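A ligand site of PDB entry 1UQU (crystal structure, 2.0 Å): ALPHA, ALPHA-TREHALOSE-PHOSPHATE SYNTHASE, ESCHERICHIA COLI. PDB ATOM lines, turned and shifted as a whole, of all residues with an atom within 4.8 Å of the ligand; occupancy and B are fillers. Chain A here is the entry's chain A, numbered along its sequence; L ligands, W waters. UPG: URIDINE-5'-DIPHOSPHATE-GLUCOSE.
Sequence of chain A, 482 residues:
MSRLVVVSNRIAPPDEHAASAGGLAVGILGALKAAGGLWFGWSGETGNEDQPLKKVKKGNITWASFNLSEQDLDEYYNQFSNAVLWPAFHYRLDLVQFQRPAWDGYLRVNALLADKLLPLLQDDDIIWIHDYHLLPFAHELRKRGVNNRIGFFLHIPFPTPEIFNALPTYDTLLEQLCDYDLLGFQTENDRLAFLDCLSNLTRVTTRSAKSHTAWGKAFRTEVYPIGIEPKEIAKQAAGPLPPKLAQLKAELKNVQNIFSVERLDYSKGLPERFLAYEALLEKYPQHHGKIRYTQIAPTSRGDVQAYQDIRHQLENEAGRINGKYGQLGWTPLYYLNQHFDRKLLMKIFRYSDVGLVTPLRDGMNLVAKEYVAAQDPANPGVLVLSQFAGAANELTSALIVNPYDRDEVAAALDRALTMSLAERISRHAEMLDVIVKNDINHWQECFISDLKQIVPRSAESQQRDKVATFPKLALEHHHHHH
O3C of the ligand sits at hydrogen-bond distance from OE1 of Glu 370. The side-chain carboxylate (OD1) of Asp 362 lies within hydrogen-bond range of an oxygen (O3') of the ligand (2.6 Å). N of Phe 340 is in hydrogen-bond range of O4 of the ligand (3.0 Å). The backbone carbonyl oxygen (O) of Phe 340 lies within hydrogen-bond range of a nitrogen (N3) of the ligand. N of Met 364 is in hydrogen-bond range of O3' of the ligand (2.8 Å). An oxygen (O1B) of the ligand lies within salt-bridge range of the guanidinium group (NE) of Arg 263 (2.8 Å). O6' of the ligand sits at hydrogen-bond distance from ND1 of His 155 (2.8 Å). O1A of the ligand lies within hydrogen-bond range of N of Leu 366. The backbone NH (N) of Asn 365 sits at hydrogen-bond distance from an oxygen (O4') of the ligand (2.8 Å). The side-chain amino group (NZ) of Lys 268 is in salt-bridge range of an oxygen (O2B) of the ligand, at 3.0 Å. The side-chain amide oxygen (OE1) of Gln 186 is in hydrogen-bond range of an oxygen (O6') of the ligand, 3.0 Å away. O3' of the ligand is in hydrogen-bond range of N of Gly 363. ND1 of His 339 lies close to N3 of the ligand. N of Val 367 lies within hydrogen-bond range of O2A of the ligand. The guanidinium group (NE) of Arg 342 is in hydrogen-bond range of an oxygen (O3C) of the ligand (3.3 Å).
The guanidinium group (NE) of Arg 342 is in salt-bridge range of the side-chain carboxylate (OE1) of Glu 370 (2.8 Å). The side-chain carboxylate (OD2) of Asp 362 sits at hydrogen-bond distance from the side-chain amide nitrogen (ND2) of Asn 365 (2.8 Å). OD2 of Asp 362 lies within salt-bridge range of NZ of Lys 268 (2.7 Å). O of His 155 lies close to OE1 of Gln 186 (2.8 Å). N of Val 367 is in hydrogen-bond range of OD1 of Asn 365 (3.1 Å). NE2 of Gln 186 lies close to N of Ile 226 (3.0 Å). The backbone carbonyl oxygen (O) of Trp 86 is in hydrogen-bond range of a ring nitrogen (ND1) of His 90 (3.0 Å).
Trp 86 touches the ligand. CG2 of Ile 226 touches O6' of the ligand (3.5 Å). Val 261 touches the ligand. CG of Pro 298 touches O4 of the ligand (3.6 Å). Leu 345 touches the ligand. Hydrophobic or aromatic side chains that line the ligand: Trp 86, His 155, Ile 226, Val 261, Pro 298, His 339, Leu 345, Met 364, Leu 366 and Val 367.
Water W2 bridges O2A of the ligand (2.5 Å) and NZ of Lys 268 (3.0 Å). Water W1 bridges an oxygen (O3C) of the ligand (2.7 Å) and the backbone NH of Gly 23 (2.8 Å). Water W7 lies within hydrogen-bond range of O2' of the ligand (2.7 Å), N of Gly 363 (2.8 Å), NE2 of His 90 (2.8 Å) and OD1 of Asp 362 (3.2 Å). Water W6 lies within hydrogen-bond range of O1B of the ligand (2.9 Å) and N of Arg 263 (2.9 Å). Water W4 lies within hydrogen-bond range of N of Arg 342, O2 of the ligand, NE2 of His 339 and O of Phe 340.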
ATOM      1  N   GLY A  23       7.918 -28.507 -27.646  1.00  0.00           N
ATOM      2  CA  GLY A  23       8.929 -28.588 -26.600  1.00  0.00           C
ATOM      3  C   GLY A  23       9.382 -29.971 -26.197  1.00  0.00           C
ATOM      4  O   GLY A  23      10.573 -30.265 -26.224  1.00  0.00           O
ATOM      5  N   TRP A  86      -5.578 -35.687 -13.676  1.00  0.00           N
ATOM      6  CA  TRP A  86      -5.274 -34.276 -13.957  1.00  0.00           C
ATOM      7  C   TRP A  86      -5.828 -33.337 -12.846  1.00  0.00           C
ATOM      8  O   TRP A  86      -5.055 -32.598 -12.285  1.00  0.00           O
ATOM      9  CB  TRP A  86      -5.703 -33.805 -15.363  1.00  0.00           C
ATOM     10  CG  TRP A  86      -5.294 -32.372 -15.657  1.00  0.00           C
ATOM     11  CD1 TRP A  86      -5.995 -31.223 -15.357  1.00  0.00           C
ATOM     12  CD2 TRP A  86      -4.077 -31.939 -16.287  1.00  0.00           C
ATOM     13  NE1 TRP A  86      -5.280 -30.116 -15.751  1.00  0.00           N
ATOM     14  CE2 TRP A  86      -4.106 -30.524 -16.333  1.00  0.00           C
ATOM     15  CE3 TRP A  86      -2.952 -32.611 -16.824  1.00  0.00           C
ATOM     16  CZ2 TRP A  86      -3.056 -29.769 -16.884  1.00  0.00           C
ATOM     17  CZ3 TRP A  86      -1.916 -31.854 -17.395  1.00  0.00           C
ATOM     18  CH2 TRP A  86      -1.977 -30.443 -17.417  1.00  0.00           C
ATOM     19  N   HIS A  90      -3.380 -31.520  -9.936  1.00  0.00           N
ATOM     20  CA  HIS A  90      -3.421 -30.067  -9.861  1.00  0.00           C
ATOM     21  C   HIS A  90      -4.227 -29.502  -8.694  1.00  0.00           C
ATOM     22  O   HIS A  90      -4.666 -28.342  -8.741  1.00  0.00           O
ATOM     23  CB  HIS A  90      -3.891 -29.453 -11.178  1.00  0.00           C
ATOM     24  CG  HIS A  90      -2.891 -29.628 -12.279  1.00  0.00           C
ATOM     25  ND1 HIS A  90      -2.762 -30.819 -12.978  1.00  0.00           N
ATOM     26  CD2 HIS A  90      -1.954 -28.801 -12.772  1.00  0.00           C
ATOM     27  CE1 HIS A  90      -1.794 -30.694 -13.860  1.00  0.00           C
ATOM     28  NE2 HIS A  90      -1.287 -29.480 -13.765  1.00  0.00           N
ATOM     29  N   HIS A 155       5.334 -35.014 -16.049  1.00  0.00           N
ATOM     30  CA  HIS A 155       5.426 -33.667 -16.577  1.00  0.00           C
ATOM     31  C   HIS A 155       4.618 -32.665 -15.730  1.00  0.00           C
ATOM     32  O   HIS A 155       4.775 -31.440 -15.866  1.00  0.00           O
ATOM     33  CB  HIS A 155       4.984 -33.623 -18.050  1.00  0.00           C
ATOM     34  CG  HIS A 155       5.941 -34.303 -18.981  1.00  0.00           C
ATOM     35  ND1 HIS A 155       6.887 -33.609 -19.721  1.00  0.00           N
ATOM     36  CD2 HIS A 155       6.133 -35.622 -19.280  1.00  0.00           C
ATOM     37  CE1 HIS A 155       7.606 -34.461 -20.437  1.00  0.00           C
ATOM     38  NE2 HIS A 155       7.159 -35.691 -20.203  1.00  0.00           N
ATOM     39  N   ILE A 156       3.795 -33.179 -14.840  1.00  0.00           N
ATOM     40  CA  ILE A 156       2.884 -32.344 -14.030  1.00  0.00           C
ATOM     41  C   ILE A 156       3.278 -32.467 -12.570  1.00  0.00           C
ATOM     42  O   ILE A 156       4.140 -33.297 -12.234  1.00  0.00           O
ATOM     43  CB  ILE A 156       1.401 -32.738 -14.263  1.00  0.00           C
ATOM     44  CG1 ILE A 156       1.082 -34.105 -13.633  1.00  0.00           C
ATOM     45  CG2 ILE A 156       1.047 -32.677 -15.733  1.00  0.00           C
ATOM     46  CD1 ILE A 156      -0.383 -34.462 -13.685  1.00  0.00           C
ATOM     47  N   GLN A 186       9.529 -32.681 -12.232  1.00  0.00           N
ATOM     48  CA  GLN A 186       9.851 -31.318 -12.654  1.00  0.00           C
ATOM     49  C   GLN A 186      10.549 -30.475 -11.582  1.00  0.00           C
ATOM     50  O   GLN A 186      11.331 -29.603 -11.918  1.00  0.00           O
ATOM     51  CB  GLN A 186       8.584 -30.589 -13.091  1.00  0.00           C
ATOM     52  CG  GLN A 186       7.845 -31.307 -14.241  1.00  0.00           C
ATOM     53  CD  GLN A 186       8.255 -30.792 -15.615  1.00  0.00           C
ATOM     54  OE1 GLN A 186       7.423 -30.717 -16.513  1.00  0.00           O
ATOM     55  NE2 GLN A 186       9.500 -30.375 -15.753  1.00  0.00           N
ATOM     56  N   ILE A 226      12.009 -29.521 -17.226  1.00  0.00           N
ATOM     57  CA  ILE A 226      12.033 -29.522 -18.710  1.00  0.00           C
ATOM     58  C   ILE A 226      12.289 -28.110 -19.223  1.00  0.00           C
ATOM     59  O   ILE A 226      11.882 -27.113 -18.591  1.00  0.00           O
ATOM     60  CB  ILE A 226      10.730 -30.096 -19.308  1.00  0.00           C
ATOM     61  CG1 ILE A 226      10.952 -30.563 -20.773  1.00  0.00           C
ATOM     62  CG2 ILE A 226       9.562 -29.105 -19.213  1.00  0.00           C
ATOM     63  CD1 ILE A 226       9.789 -31.339 -21.348  1.00  0.00           C
ATOM     64  N   VAL A 261      -0.428 -17.187 -23.734  1.00  0.00           N
ATOM     65  CA  VAL A 261      -0.887 -18.347 -24.499  1.00  0.00           C
ATOM     66  C   VAL A 261      -0.758 -19.617 -23.661  1.00  0.00           C
ATOM     67  O   VAL A 261       0.222 -19.828 -22.954  1.00  0.00           O
ATOM     68  CB  VAL A 261      -0.133 -18.503 -25.874  1.00  0.00           C
ATOM     69  CG1 VAL A 261       1.368 -18.469 -25.686  1.00  0.00           C
ATOM     70  CG2 VAL A 261      -0.544 -19.804 -26.558  1.00  0.00           C
ATOM     71  N   GLU A 262      -1.812 -20.433 -23.710  1.00  0.00           N
ATOM     72  CA  GLU A 262      -1.776 -21.789 -23.153  1.00  0.00           C
ATOM     73  C   GLU A 262      -2.984 -22.558 -23.640  1.00  0.00           C
ATOM     74  O   GLU A 262      -3.928 -21.969 -24.138  1.00  0.00           O
ATOM     75  CB  GLU A 262      -1.830 -21.805 -21.627  1.00  0.00           C
ATOM     76  CG  GLU A 262      -2.840 -20.846 -21.018  1.00  0.00           C
ATOM     77  CD  GLU A 262      -2.136 -19.642 -20.471  1.00  0.00           C
ATOM     78  OE1 GLU A 262      -1.607 -19.746 -19.340  1.00  0.00           O
ATOM     79  OE2 GLU A 262      -2.057 -18.610 -21.195  1.00  0.00           O
ATOM     80  N   ARG A 263      -2.953 -23.863 -23.455  1.00  0.00           N
ATOM     81  CA  ARG A 263      -4.186 -24.642 -23.562  1.00  0.00           C
ATOM     82  C   ARG A 263      -5.224 -24.038 -22.612  1.00  0.00           C
ATOM     83  O   ARG A 263      -4.885 -23.597 -21.495  1.00  0.00           O
ATOM     84  CB  ARG A 263      -3.969 -26.102 -23.133  1.00  0.00           C
ATOM     85  CG  ARG A 263      -3.063 -26.988 -24.025  1.00  0.00           C
ATOM     86  CD  ARG A 263      -2.895 -28.404 -23.489  1.00  0.00           C
ATOM     87  NE  ARG A 263      -2.387 -28.330 -22.119  1.00  0.00           N
ATOM     88  CZ  ARG A 263      -3.137 -28.400 -21.009  1.00  0.00           C
ATOM     89  NH1 ARG A 263      -4.460 -28.619 -21.076  1.00  0.00           N
ATOM     90  NH2 ARG A 263      -2.562 -28.259 -19.839  1.00  0.00           N
ATOM     91  N   LYS A 268      -4.533 -23.226 -15.460  1.00  0.00           N
ATOM     92  CA  LYS A 268      -3.825 -22.027 -15.917  1.00  0.00           C
ATOM     93  C   LYS A 268      -4.343 -20.703 -15.320  1.00  0.00           C
ATOM     94  O   LYS A 268      -3.737 -19.678 -15.524  1.00  0.00           O
ATOM     95  CB  LYS A 268      -3.850 -21.937 -17.442  1.00  0.00           C
ATOM     96  CG  LYS A 268      -3.349 -23.176 -18.188  1.00  0.00           C
ATOM     97  CD  LYS A 268      -1.822 -23.387 -18.003  1.00  0.00           C
ATOM     98  CE  LYS A 268      -1.394 -24.714 -18.620  1.00  0.00           C
ATOM     99  NZ  LYS A 268       0.100 -24.906 -18.778  1.00  0.00           N
ATOM    100  N   ILE A 296      -4.423 -16.181 -26.038  1.00  0.00           N
ATOM    101  CA  ILE A 296      -4.661 -17.273 -26.980  1.00  0.00           C
ATOM    102  C   ILE A 296      -4.841 -18.511 -26.121  1.00  0.00           C
ATOM    103  O   ILE A 296      -4.068 -18.749 -25.205  1.00  0.00           O
ATOM    104  CB  ILE A 296      -3.461 -17.379 -27.969  1.00  0.00           C
ATOM    105  CG1 ILE A 296      -3.423 -16.152 -28.883  1.00  0.00           C
ATOM    106  CG2 ILE A 296      -3.529 -18.703 -28.782  1.00  0.00           C
ATOM    107  CD1 ILE A 296      -2.139 -16.001 -29.681  1.00  0.00           C
ATOM    108  N   PRO A 298      -6.426 -22.234 -27.059  1.00  0.00           N
ATOM    109  CA  PRO A 298      -7.124 -23.264 -27.836  1.00  0.00           C
ATOM    110  C   PRO A 298      -7.799 -24.231 -26.879  1.00  0.00           C
ATOM    111  O   PRO A 298      -7.310 -24.494 -25.777  1.00  0.00           O
ATOM    112  CB  PRO A 298      -6.003 -23.969 -28.617  1.00  0.00           C
ATOM    113  CG  PRO A 298      -4.714 -23.683 -27.829  1.00  0.00           C
ATOM    114  CD  PRO A 298      -4.958 -22.315 -27.196  1.00  0.00           C
ATOM    115  N   GLN A 338      -8.219 -20.373 -30.128  1.00  0.00           N
ATOM    116  CA  GLN A 338      -7.625 -20.806 -31.379  1.00  0.00           C
ATOM    117  C   GLN A 338      -6.203 -21.295 -31.149  1.00  0.00           C
ATOM    118  O   GLN A 338      -5.520 -20.817 -30.279  1.00  0.00           O
ATOM    119  CB  GLN A 338      -7.594 -19.623 -32.369  1.00  0.00           C
ATOM    120  CG  GLN A 338      -8.980 -19.214 -32.900  1.00  0.00           C
ATOM    121  CD  GLN A 338      -8.902 -17.891 -33.668  1.00  0.00           C
ATOM    122  OE1 GLN A 338      -7.960 -17.696 -34.467  1.00  0.00           O
ATOM    123  NE2 GLN A 338      -9.866 -16.988 -33.433  1.00  0.00           N
ATOM    124  N   HIS A 339      -5.768 -22.241 -31.941  1.00  0.00           N
ATOM    125  CA  HIS A 339      -4.407 -22.752 -31.779  1.00  0.00           C
ATOM    126  C   HIS A 339      -3.508 -22.036 -32.775  1.00  0.00           C
ATOM    127  O   HIS A 339      -3.888 -21.824 -33.946  1.00  0.00           O
ATOM    128  CB  HIS A 339      -4.381 -24.270 -31.970  1.00  0.00           C
ATOM    129  CG  HIS A 339      -2.999 -24.846 -32.070  1.00  0.00           C
ATOM    130  ND1 HIS A 339      -2.292 -25.287 -30.968  1.00  0.00           N
ATOM    131  CD2 HIS A 339      -2.211 -25.087 -33.152  1.00  0.00           C
ATOM    132  CE1 HIS A 339      -1.125 -25.762 -31.365  1.00  0.00           C
ATOM    133  NE2 HIS A 339      -1.056 -25.652 -32.686  1.00  0.00           N
ATOM    134  N   PHE A 340      -2.326 -21.657 -32.311  1.00  0.00           N
ATOM    135  CA  PHE A 340      -1.353 -20.932 -33.110  1.00  0.00           C
ATOM    136  C   PHE A 340      -0.102 -21.805 -33.242  1.00  0.00           C
ATOM    137  O   PHE A 340       0.304 -22.452 -32.260  1.00  0.00           O
ATOM    138  CB  PHE A 340      -0.987 -19.618 -32.392  1.00  0.00           C
ATOM    139  CG  PHE A 340      -1.905 -18.459 -32.705  1.00  0.00           C
ATOM    140  CD1 PHE A 340      -3.285 -18.543 -32.430  1.00  0.00           C
ATOM    141  CD2 PHE A 340      -1.407 -17.292 -33.273  1.00  0.00           C
ATOM    142  CE1 PHE A 340      -4.132 -17.494 -32.737  1.00  0.00           C
ATOM    143  CE2 PHE A 340      -2.259 -16.213 -33.584  1.00  0.00           C
ATOM    144  CZ  PHE A 340      -3.624 -16.321 -33.325  1.00  0.00           C
ATOM    145  N   ASP A 341       0.504 -21.846 -34.432  1.00  0.00           N
ATOM    146  CA  ASP A 341       1.783 -22.531 -34.603  1.00  0.00           C
ATOM    147  C   ASP A 341       2.859 -21.987 -33.642  1.00  0.00           C
ATOM    148  O   ASP A 341       2.923 -20.772 -33.387  1.00  0.00           O
ATOM    149  CB  ASP A 341       2.282 -22.407 -36.044  1.00  0.00           C
ATOM    150  CG  ASP A 341       3.479 -23.283 -36.311  1.00  0.00           C
ATOM    151  OD1 ASP A 341       4.626 -22.785 -36.211  1.00  0.00           O
ATOM    152  OD2 ASP A 341       3.389 -24.503 -36.584  1.00  0.00           O
ATOM    153  N   ARG A 342       3.678 -22.894 -33.089  1.00  0.00           N
ATOM    154  CA  ARG A 342       4.725 -22.545 -32.112  1.00  0.00           C
ATOM    155  C   ARG A 342       5.803 -21.601 -32.702  1.00  0.00           C
ATOM    156  O   ARG A 342       6.271 -20.679 -32.031  1.00  0.00           O
ATOM    157  CB  ARG A 342       5.391 -23.825 -31.586  1.00  0.00           C
ATOM    158  CG  ARG A 342       6.265 -23.663 -30.344  1.00  0.00           C
ATOM    159  CD  ARG A 342       6.721 -24.979 -29.739  1.00  0.00           C
ATOM    160  NE  ARG A 342       7.598 -24.770 -28.599  1.00  0.00           N
ATOM    161  CZ  ARG A 342       8.847 -25.218 -28.493  1.00  0.00           C
ATOM    162  NH1 ARG A 342       9.394 -25.940 -29.469  1.00  0.00           N
ATOM    163  NH2 ARG A 342       9.534 -24.964 -27.377  1.00  0.00           N
ATOM    164  N   LEU A 345       4.300 -18.217 -32.658  1.00  0.00           N
ATOM    165  CA  LEU A 345       4.240 -17.714 -31.284  1.00  0.00           C
ATOM    166  C   LEU A 345       5.557 -17.074 -30.837  1.00  0.00           C
ATOM    167  O   LEU A 345       5.568 -16.093 -30.092  1.00  0.00           O
ATOM    168  CB  LEU A 345       3.850 -18.837 -30.303  1.00  0.00           C
ATOM    169  CG  LEU A 345       2.377 -19.263 -30.247  1.00  0.00           C
ATOM    170  CD1 LEU A 345       2.208 -20.479 -29.301  1.00  0.00           C
ATOM    171  CD2 LEU A 345       1.492 -18.124 -29.814  1.00  0.00           C
ATOM    172  N   MET A 346       6.670 -17.665 -31.271  1.00  0.00           N
ATOM    173  CA  MET A 346       7.988 -17.126 -30.908  1.00  0.00           C
ATOM    174  C   MET A 346       8.134 -15.714 -31.418  1.00  0.00           C
ATOM    175  O   MET A 346       8.624 -14.836 -30.705  1.00  0.00           O
ATOM    176  CB  MET A 346       9.116 -18.014 -31.491  1.00  0.00           C
ATOM    177  CG  MET A 346       9.149 -19.448 -30.923  1.00  0.00           C
ATOM    178  SD  MET A 346       8.935 -19.638 -29.158  1.00  0.00           S
ATOM    179  CE  MET A 346       7.212 -20.016 -29.006  1.00  0.00           C
ATOM    180  N   ASP A 362       1.313 -25.481 -12.117  1.00  0.00           N
ATOM    181  CA  ASP A 362       1.856 -25.922 -13.404  1.00  0.00           C
ATOM    182  C   ASP A 362       3.132 -26.713 -13.142  1.00  0.00           C
ATOM    183  O   ASP A 362       4.002 -26.233 -12.442  1.00  0.00           O
ATOM    184  CB  ASP A 362       2.144 -24.735 -14.331  1.00  0.00           C
ATOM    185  CG  ASP A 362       1.677 -24.980 -15.771  1.00  0.00           C
ATOM    186  OD1 ASP A 362       1.606 -26.155 -16.184  1.00  0.00           O
ATOM    187  OD2 ASP A 362       1.355 -24.055 -16.556  1.00  0.00           O
ATOM    188  N   GLY A 363       3.233 -27.927 -13.698  1.00  0.00           N
ATOM    189  CA  GLY A 363       4.437 -28.725 -13.556  1.00  0.00           C
ATOM    190  C   GLY A 363       5.685 -27.890 -13.820  1.00  0.00           C
ATOM    191  O   GLY A 363       6.608 -27.856 -13.007  1.00  0.00           O
ATOM    192  N   MET A 364       5.713 -27.194 -14.946  1.00  0.00           N
ATOM    193  CA  MET A 364       6.847 -26.330 -15.242  1.00  0.00           C
ATOM    194  C   MET A 364       6.354 -25.038 -15.844  1.00  0.00           C
ATOM    195  O   MET A 364       6.444 -23.941 -15.259  1.00  0.00           O
ATOM    196  CB  MET A 364       7.808 -27.047 -16.222  1.00  0.00           C
ATOM    197  CG  MET A 364       9.033 -26.218 -16.594  1.00  0.00           C
ATOM    198  SD  MET A 364      10.060 -26.015 -15.127  1.00  0.00           S
ATOM    199  CE  MET A 364      10.414 -24.694 -15.290  1.00  0.00           C
ATOM    200  N   ASN A 365       5.801 -25.211 -17.050  1.00  0.00           N
ATOM    201  CA  ASN A 365       5.319 -24.175 -17.943  1.00  0.00           C
ATOM    202  C   ASN A 365       6.407 -23.724 -18.892  1.00  0.00           C
ATOM    203  O   ASN A 365       7.285 -22.917 -18.570  1.00  0.00           O
ATOM    204  CB  ASN A 365       4.612 -23.018 -17.220  1.00  0.00           C
ATOM    205  CG  ASN A 365       3.861 -22.106 -18.181  1.00  0.00           C
ATOM    206  OD1 ASN A 365       4.475 -21.530 -19.075  1.00  0.00           O
ATOM    207  ND2 ASN A 365       2.524 -21.976 -18.003  1.00  0.00           N
ATOM    208  N   LEU A 366       6.375 -24.298 -20.085  1.00  0.00           N
ATOM    209  CA  LEU A 366       7.336 -23.974 -21.106  1.00  0.00           C
ATOM    210  C   LEU A 366       7.110 -22.595 -21.724  1.00  0.00           C
ATOM    211  O   LEU A 366       8.039 -21.965 -22.146  1.00  0.00           O
ATOM    212  CB  LEU A 366       7.330 -25.034 -22.210  1.00  0.00           C
ATOM    213  CG  LEU A 366       8.074 -26.334 -21.857  1.00  0.00           C
ATOM    214  CD1 LEU A 366       8.228 -27.139 -23.121  1.00  0.00           C
ATOM    215  CD2 LEU A 366       9.434 -26.068 -21.276  1.00  0.00           C
ATOM    216  N   VAL A 367       5.877 -22.126 -21.756  1.00  0.00           N
ATOM    217  CA  VAL A 367       5.598 -20.833 -22.350  1.00  0.00           C
ATOM    218  C   VAL A 367       6.456 -19.754 -21.711  1.00  0.00           C
ATOM    219  O   VAL A 367       6.908 -18.832 -22.395  1.00  0.00           O
ATOM    220  CB  VAL A 367       4.081 -20.468 -22.275  1.00  0.00           C
ATOM    221  CG1 VAL A 367       3.833 -18.943 -22.446  1.00  0.00           C
ATOM    222  CG2 VAL A 367       3.306 -21.224 -23.345  1.00  0.00           C
ATOM    223  N   GLU A 370       9.930 -20.004 -23.078  1.00  0.00           N
ATOM    224  CA  GLU A 370       9.901 -19.612 -24.503  1.00  0.00           C
ATOM    225  C   GLU A 370       9.871 -18.107 -24.656  1.00  0.00           C
ATOM    226  O   GLU A 370      10.547 -17.531 -25.517  1.00  0.00           O
ATOM    227  CB  GLU A 370       8.664 -20.196 -25.212  1.00  0.00           C
ATOM    228  CG  GLU A 370       8.758 -21.702 -25.461  1.00  0.00           C
ATOM    229  CD  GLU A 370       7.437 -22.410 -25.783  1.00  0.00           C
ATOM    230  OE1 GLU A 370       7.439 -23.641 -26.018  1.00  0.00           O
ATOM    231  OE2 GLU A 370       6.392 -21.766 -25.828  1.00  0.00           O
HETATM  232  N1  UPG L   1       1.466 -24.014 -27.701  1.00  0.00           N
HETATM  233  C2  UPG L   1       1.348 -23.931 -29.102  1.00  0.00           C
HETATM  234  N3  UPG L   1       0.208 -23.398 -29.696  1.00  0.00           N
HETATM  235  C4  UPG L   1      -0.839 -22.959 -28.883  1.00  0.00           C
HETATM  236  C5  UPG L   1      -0.753 -23.080 -27.492  1.00  0.00           C
HETATM  237  C6  UPG L   1       0.407 -23.601 -26.891  1.00  0.00           C
HETATM  238  O2  UPG L   1       2.310 -24.222 -29.798  1.00  0.00           O
HETATM  239  O4  UPG L   1      -1.764 -22.296 -29.431  1.00  0.00           O
HETATM  240  C1C UPG L   1       2.685 -24.608 -27.186  1.00  0.00           C
HETATM  241  C2C UPG L   1       3.460 -23.678 -26.333  1.00  0.00           C
HETATM  242  O2C UPG L   1       4.244 -22.829 -27.109  1.00  0.00           O
HETATM  243  C3C UPG L   1       4.226 -24.643 -25.476  1.00  0.00           C
HETATM  244  C4C UPG L   1       3.222 -25.781 -25.262  1.00  0.00           C
HETATM  245  O4C UPG L   1       2.249 -25.620 -26.299  1.00  0.00           O
HETATM  246  O3C UPG L   1       5.424 -25.148 -26.095  1.00  0.00           O
HETATM  247  C5C UPG L   1       2.556 -25.651 -23.897  1.00  0.00           C
HETATM  248  O5C UPG L   1       3.390 -26.310 -22.958  1.00  0.00           O
HETATM  249  PA  UPG L   1       3.330 -25.719 -21.452  1.00  0.00           P
HETATM  250  O1A UPG L   1       4.455 -26.269 -20.749  1.00  0.00           O
HETATM  251  O2A UPG L   1       3.314 -24.220 -21.454  1.00  0.00           O
HETATM  252  O3A UPG L   1       1.932 -26.152 -20.886  1.00  0.00           O
HETATM  253  PB  UPG L   1       1.280 -27.574 -20.903  1.00  0.00           P
HETATM  254  O1B UPG L   1       0.290 -27.704 -22.009  1.00  0.00           O
HETATM  255  O2B UPG L   1       0.365 -27.700 -19.694  1.00  0.00           O
HETATM  256  O3B UPG L   1       1.884 -29.041 -20.922  1.00  0.00           O
HETATM  257  C1' UPG L   1       2.138 -29.885 -19.705  1.00  0.00           C
HETATM  258  C2' UPG L   1       2.414 -29.496 -18.312  1.00  0.00           C
HETATM  259  C3' UPG L   1       3.456 -28.249 -18.159  1.00  0.00           C
HETATM  260  C4' UPG L   1       4.855 -28.700 -18.695  1.00  0.00           C
HETATM  261  C5' UPG L   1       4.663 -29.394 -20.225  1.00  0.00           C
HETATM  262  C6' UPG L   1       5.976 -30.229 -20.525  1.00  0.00           C
HETATM  263  O2' UPG L   1       1.180 -29.080 -17.739  1.00  0.00           O
HETATM  264  O3' UPG L   1       3.703 -27.550 -16.791  1.00  0.00           O
HETATM  265  O4' UPG L   1       5.735 -27.437 -18.807  1.00  0.00           O
HETATM  266  O5' UPG L   1       3.550 -30.313 -20.077  1.00  0.00           O
HETATM  267  O6' UPG L   1       6.555 -30.859 -19.377  1.00  0.00           O
HETATM  268  O   HOH W   1       5.300 -27.508 -27.371  1.00  0.00           O
HETATM  269  O   HOH W   2       1.090 -23.125 -20.999  1.00  0.00           O
HETATM  270  O   HOH W   3       1.295 -32.977 -19.203  1.00  0.00           O
HETATM  271  O   HOH W   4       2.250 -25.341 -32.558  1.00  0.00           O
HETATM  272  O   HOH W   5       3.733 -29.648 -23.799  1.00  0.00           O
HETATM  273  O   HOH W   6      -0.474 -24.911 -22.327  1.00  0.00           O
HETATM  274  O   HOH W   7       1.148 -29.134 -15.043  1.00  0.00           O
